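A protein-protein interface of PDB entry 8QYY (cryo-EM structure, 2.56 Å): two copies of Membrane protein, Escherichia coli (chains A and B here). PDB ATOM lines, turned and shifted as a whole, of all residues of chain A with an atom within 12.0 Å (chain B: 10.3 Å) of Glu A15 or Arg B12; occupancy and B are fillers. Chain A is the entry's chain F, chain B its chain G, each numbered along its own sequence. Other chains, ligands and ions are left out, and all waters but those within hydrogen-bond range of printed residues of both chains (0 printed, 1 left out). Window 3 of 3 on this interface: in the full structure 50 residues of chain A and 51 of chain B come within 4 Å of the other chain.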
ATOM      1  N   VAL A   8       5.077 -14.452  34.705  1.00  0.00           N
ATOM      2  CA  VAL A   8       5.554 -14.643  33.341  1.00  0.00           C
ATOM      3  C   VAL A   8       4.487 -14.189  32.352  1.00  0.00           C
ATOM      4  O   VAL A   8       3.276 -14.314  32.595  1.00  0.00           O
ATOM      5  CB  VAL A   8       5.951 -16.112  33.104  1.00  0.00           C
ATOM      6  CG1 VAL A   8       6.988 -16.553  34.126  1.00  0.00           C
ATOM      7  CG2 VAL A   8       4.729 -17.019  33.160  1.00  0.00           C
ATOM      8  N   LYS A   9       4.937 -13.637  31.229  1.00  0.00           N
ATOM      9  CA  LYS A   9       4.049 -13.128  30.195  1.00  0.00           C
ATOM     10  C   LYS A   9       4.566 -13.607  28.843  1.00  0.00           C
ATOM     11  O   LYS A   9       5.513 -14.396  28.764  1.00  0.00           O
ATOM     12  CB  LYS A   9       3.947 -11.598  30.271  1.00  0.00           C
ATOM     13  CG  LYS A   9       2.633 -11.083  30.835  1.00  0.00           C
ATOM     14  CD  LYS A   9       2.609 -11.145  32.352  1.00  0.00           C
ATOM     15  CE  LYS A   9       1.236 -10.778  32.892  1.00  0.00           C
ATOM     16  NZ  LYS A   9       1.172 -10.899  34.376  1.00  0.00           N
ATOM     17  N   LYS A  10       3.923 -13.131  27.774  1.00  0.00           N
ATOM     18  CA  LYS A  10       4.315 -13.432  26.396  1.00  0.00           C
ATOM     19  C   LYS A  10       4.293 -14.934  26.116  1.00  0.00           C
ATOM     20  O   LYS A  10       5.004 -15.429  25.240  1.00  0.00           O
ATOM     21  CB  LYS A  10       5.693 -12.839  26.072  1.00  0.00           C
ATOM     22  CG  LYS A  10       5.970 -12.622  24.586  1.00  0.00           C
ATOM     23  CD  LYS A  10       7.428 -12.893  24.240  1.00  0.00           C
ATOM     24  CE  LYS A  10       7.760 -14.372  24.346  1.00  0.00           C
ATOM     25  NZ  LYS A  10       9.016 -14.725  23.634  1.00  0.00           N
ATOM     26  N   ARG A  11       3.464 -15.679  26.845  1.00  0.00           N
ATOM     27  CA  ARG A  11       3.361 -17.113  26.616  1.00  0.00           C
ATOM     28  C   ARG A  11       2.583 -17.358  25.331  1.00  0.00           C
ATOM     29  O   ARG A  11       1.410 -17.746  25.365  1.00  0.00           O
ATOM     30  CB  ARG A  11       2.696 -17.801  27.810  1.00  0.00           C
ATOM     31  CG  ARG A  11       2.709 -19.319  27.756  1.00  0.00           C
ATOM     32  CD  ARG A  11       1.759 -19.901  28.789  1.00  0.00           C
ATOM     33  NE  ARG A  11       2.064 -19.416  30.130  1.00  0.00           N
ATOM     34  CZ  ARG A  11       1.176 -19.319  31.110  1.00  0.00           C
ATOM     35  NH1 ARG A  11      -0.089 -19.660  30.933  1.00  0.00           N
ATOM     36  NH2 ARG A  11       1.569 -18.863  32.296  1.00  0.00           N
ATOM     37  N   ARG A  12       3.230 -17.122  24.190  1.00  0.00           N
ATOM     38  CA  ARG A  12       2.560 -17.130  22.889  1.00  0.00           C
ATOM     39  C   ARG A  12       3.562 -17.624  21.849  1.00  0.00           C
ATOM     40  O   ARG A  12       4.419 -16.861  21.393  1.00  0.00           O
ATOM     41  CB  ARG A  12       2.027 -15.740  22.553  1.00  0.00           C
ATOM     42  CG  ARG A  12       1.181 -15.640  21.289  1.00  0.00           C
ATOM     43  CD  ARG A  12       2.014 -15.272  20.069  1.00  0.00           C
ATOM     44  NE  ARG A  12       1.187 -15.025  18.893  1.00  0.00           N
ATOM     45  CZ  ARG A  12       1.663 -14.847  17.668  1.00  0.00           C
ATOM     46  NH1 ARG A  12       2.962 -14.872  17.422  1.00  0.00           N
ATOM     47  NH2 ARG A  12       0.814 -14.633  16.667  1.00  0.00           N
ATOM     48  N   SER A  13       3.458 -18.898  21.489  1.00  0.00           N
ATOM     49  CA  SER A  13       4.290 -19.444  20.426  1.00  0.00           C
ATOM     50  C   SER A  13       3.780 -18.963  19.075  1.00  0.00           C
ATOM     51  O   SER A  13       2.577 -19.006  18.801  1.00  0.00           O
ATOM     52  CB  SER A  13       4.295 -20.972  20.483  1.00  0.00           C
ATOM     53  OG  SER A  13       2.987 -21.495  20.331  1.00  0.00           O
ATOM     54  N   ASP A  14       4.696 -18.497  18.232  1.00  0.00           N
ATOM     55  CA  ASP A  14       4.311 -17.963  16.934  1.00  0.00           C
ATOM     56  C   ASP A  14       3.796 -19.070  16.023  1.00  0.00           C
ATOM     57  O   ASP A  14       4.333 -20.181  16.002  1.00  0.00           O
ATOM     58  CB  ASP A  14       5.495 -17.254  16.284  1.00  0.00           C
ATOM     59  CG  ASP A  14       6.046 -16.140  17.148  1.00  0.00           C
ATOM     60  OD1 ASP A  14       6.844 -16.433  18.062  1.00  0.00           O
ATOM     61  OD2 ASP A  14       5.676 -14.969  16.916  1.00  0.00           O
ATOM     62  N   GLU A  15       2.742 -18.762  15.275  1.00  0.00           N
ATOM     63  CA  GLU A  15       2.177 -19.715  14.332  1.00  0.00           C
ATOM     64  C   GLU A  15       3.055 -19.826  13.096  1.00  0.00           C
ATOM     65  O   GLU A  15       3.547 -18.825  12.568  1.00  0.00           O
ATOM     66  CB  GLU A  15       0.761 -19.301  13.930  1.00  0.00           C
ATOM     67  CG  GLU A  15      -0.237 -19.358  15.067  1.00  0.00           C
ATOM     68  CD  GLU A  15      -0.486 -20.774  15.542  1.00  0.00           C
ATOM     69  OE1 GLU A  15      -0.411 -21.704  14.713  1.00  0.00           O
ATOM     70  OE2 GLU A  15      -0.754 -20.957  16.748  1.00  0.00           O
ATOM     71  N   ALA A  16       3.244 -21.056  12.630  1.00  0.00           N
ATOM     72  CA  ALA A  16       4.052 -21.303  11.448  1.00  0.00           C
ATOM     73  C   ALA A  16       3.288 -20.922  10.188  1.00  0.00           C
ATOM     74  O   ALA A  16       2.060 -21.031  10.129  1.00  0.00           O
ATOM     75  CB  ALA A  16       4.465 -22.771  11.384  1.00  0.00           C
ATOM     76  N   GLU A  17       4.029 -20.473   9.178  1.00  0.00           N
ATOM     77  CA  GLU A  17       3.427 -20.088   7.909  1.00  0.00           C
ATOM     78  C   GLU A  17       2.794 -21.292   7.226  1.00  0.00           C
ATOM     79  O   GLU A  17       3.371 -22.382   7.199  1.00  0.00           O
ATOM     80  CB  GLU A  17       4.487 -19.461   7.004  1.00  0.00           C
ATOM     81  CG  GLU A  17       4.010 -19.150   5.600  1.00  0.00           C
ATOM     82  CD  GLU A  17       3.340 -17.798   5.495  1.00  0.00           C
ATOM     83  OE1 GLU A  17       3.130 -17.150   6.541  1.00  0.00           O
ATOM     84  OE2 GLU A  17       3.022 -17.385   4.360  1.00  0.00           O
ATOM     85  N   LYS A  18       1.604 -21.092   6.673  1.00  0.00           N
ATOM     86  CA  LYS A  18       0.937 -22.141   5.917  1.00  0.00           C
ATOM     87  C   LYS A  18       1.596 -22.256   4.548  1.00  0.00           C
ATOM     88  O   LYS A  18       1.577 -21.286   3.781  1.00  0.00           O
ATOM     89  CB  LYS A  18      -0.545 -21.827   5.770  1.00  0.00           C
ATOM     90  CG  LYS A  18      -1.291 -21.704   7.084  1.00  0.00           C
ATOM     91  CD  LYS A  18      -1.403 -23.030   7.798  1.00  0.00           C
ATOM     92  CE  LYS A  18      -2.142 -22.870   9.111  1.00  0.00           C
ATOM     93  NZ  LYS A  18      -3.568 -22.529   8.891  1.00  0.00           N
ATOM     94  N   PRO A  19       2.174 -23.399   4.196  1.00  0.00           N
ATOM     95  CA  PRO A  19       3.077 -23.439   3.041  1.00  0.00           C
ATOM     96  C   PRO A  19       2.450 -23.884   1.729  1.00  0.00           C
ATOM     97  O   PRO A  19       3.101 -23.809   0.684  1.00  0.00           O
ATOM     98  CB  PRO A  19       4.144 -24.438   3.493  1.00  0.00           C
ATOM     99  CG  PRO A  19       3.410 -25.372   4.421  1.00  0.00           C
ATOM    100  CD  PRO A  19       2.183 -24.667   4.944  1.00  0.00           C
ATOM    101  N   ILE A  22       1.448 -21.331  -1.017  1.00  0.00           N
ATOM    102  CA  ILE A  22       2.711 -20.881  -1.595  1.00  0.00           C
ATOM    103  C   ILE A  22       3.182 -21.866  -2.658  1.00  0.00           C
ATOM    104  O   ILE A  22       3.608 -21.476  -3.753  1.00  0.00           O
ATOM    105  CB  ILE A  22       3.765 -20.699  -0.489  1.00  0.00           C
ATOM    106  CG1 ILE A  22       3.243 -19.754   0.595  1.00  0.00           C
ATOM    107  CG2 ILE A  22       5.065 -20.186  -1.074  1.00  0.00           C
ATOM    108  CD1 ILE A  22       4.309 -19.248   1.535  1.00  0.00           C
ATOM    109  N   LYS B   9      -6.238 -13.928  29.555  1.00  0.00           N
ATOM    110  CA  LYS B   9      -5.300 -13.920  28.443  1.00  0.00           C
ATOM    111  C   LYS B   9      -6.026 -14.332  27.170  1.00  0.00           C
ATOM    112  O   LYS B   9      -6.906 -15.200  27.200  1.00  0.00           O
ATOM    113  CB  LYS B   9      -4.116 -14.863  28.697  1.00  0.00           C
ATOM    114  CG  LYS B   9      -2.998 -14.275  29.553  1.00  0.00           C
ATOM    115  CD  LYS B   9      -3.391 -14.189  31.021  1.00  0.00           C
ATOM    116  CE  LYS B   9      -3.500 -15.574  31.644  1.00  0.00           C
ATOM    117  NZ  LYS B   9      -3.825 -15.515  33.096  1.00  0.00           N
ATOM    118  N   LYS B  10      -5.660 -13.703  26.057  1.00  0.00           N
ATOM    119  CA  LYS B  10      -6.280 -14.008  24.777  1.00  0.00           C
ATOM    120  C   LYS B  10      -5.964 -15.443  24.364  1.00  0.00           C
ATOM    121  O   LYS B  10      -4.912 -15.991  24.698  1.00  0.00           O
ATOM    122  CB  LYS B  10      -5.789 -13.035  23.705  1.00  0.00           C
ATOM    123  CG  LYS B  10      -6.125 -11.578  23.984  1.00  0.00           C
ATOM    124  CD  LYS B  10      -7.623 -11.347  24.042  1.00  0.00           C
ATOM    125  CE  LYS B  10      -8.268 -11.557  22.684  1.00  0.00           C
ATOM    126  NZ  LYS B  10      -7.805 -10.554  21.686  1.00  0.00           N
ATOM    127  N   ARG B  11      -6.894 -16.055  23.631  1.00  0.00           N
ATOM    128  CA  ARG B  11      -6.704 -17.446  23.251  1.00  0.00           C
ATOM    129  C   ARG B  11      -5.592 -17.573  22.212  1.00  0.00           C
ATOM    130  O   ARG B  11      -5.016 -16.588  21.741  1.00  0.00           O
ATOM    131  CB  ARG B  11      -7.981 -18.055  22.668  1.00  0.00           C
ATOM    132  CG  ARG B  11      -8.423 -17.441  21.349  1.00  0.00           C
ATOM    133  CD  ARG B  11      -9.671 -18.122  20.800  1.00  0.00           C
ATOM    134  NE  ARG B  11     -10.866 -17.974  21.622  1.00  0.00           N
ATOM    135  CZ  ARG B  11     -11.719 -16.965  21.524  1.00  0.00           C
ATOM    136  NH1 ARG B  11     -11.530 -15.982  20.657  1.00  0.00           N
ATOM    137  NH2 ARG B  11     -12.797 -16.950  22.298  1.00  0.00           N
ATOM    138  N   ARG B  12      -5.299 -18.820  21.852  1.00  0.00           N
ATOM    139  CA  ARG B  12      -4.404 -19.113  20.741  1.00  0.00           C
ATOM    140  C   ARG B  12      -5.142 -18.877  19.430  1.00  0.00           C
ATOM    141  O   ARG B  12      -5.716 -19.808  18.856  1.00  0.00           O
ATOM    142  CB  ARG B  12      -3.892 -20.554  20.836  1.00  0.00           C
ATOM    143  CG  ARG B  12      -2.966 -20.980  19.709  1.00  0.00           C
ATOM    144  CD  ARG B  12      -1.668 -20.203  19.742  1.00  0.00           C
ATOM    145  NE  ARG B  12      -0.890 -20.496  20.937  1.00  0.00           N
ATOM    146  CZ  ARG B  12       0.161 -19.794  21.335  1.00  0.00           C
ATOM    147  NH1 ARG B  12       0.596 -18.754  20.643  1.00  0.00           N
ATOM    148  NH2 ARG B  12       0.793 -20.144  22.451  1.00  0.00           N
ATOM    149  N   SER B  13      -5.150 -17.633  18.959  1.00  0.00           N
ATOM    150  CA  SER B  13      -5.894 -17.248  17.762  1.00  0.00           C
ATOM    151  C   SER B  13      -4.951 -17.316  16.568  1.00  0.00           C
ATOM    152  O   SER B  13      -4.225 -16.360  16.280  1.00  0.00           O
ATOM    153  CB  SER B  13      -6.496 -15.856  17.921  1.00  0.00           C
ATOM    154  OG  SER B  13      -5.491 -14.892  18.175  1.00  0.00           O
ATOM    155  N   ASP B  14      -4.961 -18.450  15.872  1.00  0.00           N
ATOM    156  CA  ASP B  14      -4.146 -18.591  14.675  1.00  0.00           C
ATOM    157  C   ASP B  14      -4.655 -17.662  13.581  1.00  0.00           C
ATOM    158  O   ASP B  14      -5.863 -17.529  13.367  1.00  0.00           O
ATOM    159  CB  ASP B  14      -4.154 -20.042  14.188  1.00  0.00           C
ATOM    160  CG  ASP B  14      -5.499 -20.465  13.634  1.00  0.00           C
ATOM    161  OD1 ASP B  14      -6.527 -20.169  14.277  1.00  0.00           O
ATOM    162  OD2 ASP B  14      -5.530 -21.087  12.552  1.00  0.00           O
ATOM    163  N   GLU B  15      -3.727 -17.010  12.896  1.00  0.00           N
ATOM    164  CA  GLU B  15      -4.115 -16.068  11.863  1.00  0.00           C
ATOM    165  C   GLU B  15      -4.585 -16.809  10.617  1.00  0.00           C
ATOM    166  O   GLU B  15      -4.316 -17.998  10.425  1.00  0.00           O
ATOM    167  CB  GLU B  15      -2.959 -15.127  11.524  1.00  0.00           C
ATOM    168  CG  GLU B  15      -2.916 -13.873  12.386  1.00  0.00           C
ATOM    169  CD  GLU B  15      -3.883 -12.798  11.919  1.00  0.00           C
ATOM    170  OE1 GLU B  15      -4.697 -13.073  11.013  1.00  0.00           O
ATOM    171  OE2 GLU B  15      -3.831 -11.676  12.466  1.00  0.00           O
ATOM    172  N   ALA B  16      -5.309 -16.088   9.770  1.00  0.00           N
ATOM    173  CA  ALA B  16      -5.830 -16.674   8.548  1.00  0.00           C
ATOM    174  C   ALA B  16      -4.724 -16.827   7.510  1.00  0.00           C
ATOM    175  O   ALA B  16      -3.612 -16.315   7.663  1.00  0.00           O
ATOM    176  CB  ALA B  16      -6.959 -15.815   7.986  1.00  0.00           C
ATOM    177  N   GLU B  17      -5.045 -17.556   6.446  1.00  0.00           N
ATOM    178  CA  GLU B  17      -4.161 -17.626   5.292  1.00  0.00           C
ATOM    179  C   GLU B  17      -3.886 -16.224   4.764  1.00  0.00           C
ATOM    180  O   GLU B  17      -4.791 -15.391   4.672  1.00  0.00           O
ATOM    181  CB  GLU B  17      -4.790 -18.480   4.192  1.00  0.00           C
ATOM    182  CG  GLU B  17      -4.594 -19.975   4.340  1.00  0.00           C
ATOM    183  CD  GLU B  17      -3.287 -20.454   3.743  1.00  0.00           C
ATOM    184  OE1 GLU B  17      -3.056 -21.681   3.725  1.00  0.00           O
ATOM    185  OE2 GLU B  17      -2.494 -19.606   3.286  1.00  0.00           O
ATOM    186  N   LYS B  18      -2.630 -15.963   4.428  1.00  0.00           N
ATOM    187  CA  LYS B  18      -2.286 -14.675   3.849  1.00  0.00           C
ATOM    188  C   LYS B  18      -2.964 -14.543   2.490  1.00  0.00           C
ATOM    189  O   LYS B  18      -2.759 -15.397   1.615  1.00  0.00           O
ATOM    190  CB  LYS B  18      -0.773 -14.531   3.709  1.00  0.00           C
ATOM    191  CG  LYS B  18      -0.010 -14.919   4.957  1.00  0.00           C
ATOM    192  CD  LYS B  18       1.477 -14.671   4.792  1.00  0.00           C
ATOM    193  CE  LYS B  18       1.778 -13.191   4.643  1.00  0.00           C
ATOM    194  NZ  LYS B  18       3.241 -12.939   4.544  1.00  0.00           N
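The guanidinium group of Arg A12 is in salt-bridge range of the side-chain carboxylate of Asp A14.
Among the printed residues, pairs that only touch across the chains: Arg A11 with Arg B12 (3.8 Å), Arg A12 with Arg B12 (3.2 Å), Glu A15 with Arg B12 (3.2 Å), Glu A15 with Asp B14 (3.98 Å), Glu A17 with Lys B18 (3.2 Å) and Lys A18 with Glu B17 (3.2 Å).
Arg A12 touches its own counterpart, Arg B12.
Ser A13 touches Arg B12, but with the chains exchanged Arg A12 does not touch Ser B13 (5.3 Å).
Glu A15 touches Arg B12, but with the chains exchanged Arg A12 does not touch Glu B15 (5.7 Å).
Glu A17 touches Lys B18, and with the chains exchanged Lys A18 touches Glu B17.
Of the 7 pairs that touch across the chains among the printed residues, 3 have their exchanged pair printed and touching as well.
Val A8 touches none of the printed residues of chain B.
Printed residues of chain B within 4 Å of Arg A11: Arg B12.
Of chain B, only Arg B12 comes within 4 Å of Arg A12.
Ser A13 touches just one residue of chain B: Arg B12 (2.7 Å).
No residue of chain B comes within 4 Å of Asp A14.
Of the printed residues of chain B, Glu A15 touches Arg B12 (3.2 Å) and Asp B14 (3.98 Å).
Of the printed residues of chain B, Glu A17 touches Lys B18 (3.2 Å).
Printed residues of chain B within 4 Å of Lys A18: Glu B17.
Of the printed residues of chain A, Arg B12 touches Arg A11, Arg A12, Ser A13 and Glu A15.
No residue of chain A comes within 4 Å of Ser B13.
Glu B15 touches none of the printed residues of chain A.
Of the printed residues of chain A, Glu B17 touches Lys A18 (3.2 Å).
Of the printed residues of chain A, Lys B18 touches Glu A17.
The nearest residue of chain B that does not touch Glu A15 is Glu B15 (4.7 Å).
The nearest residue of chain A that does not touch Arg B12 is Asp A14 (4.8 Å).
The nearest printed residue of chain A that does not touch Lys B18 is Ile A22 (6.3 Å).
The backbone carbonyl oxygen (O) of Ser A13 sits at hydrogen-bond distance from the guanidinium group (NH1) of Arg B12, 2.7 Å away.
Of the 10 printed residues of chain B, 4 touch a printed residue of chain A.
Among the printed residues, 7 pairs touch across the chains.
Among the printed residues, no Asp or Glu carboxylate lies within 4 Å of a Lys or Arg side-chain nitrogen of the other chain.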
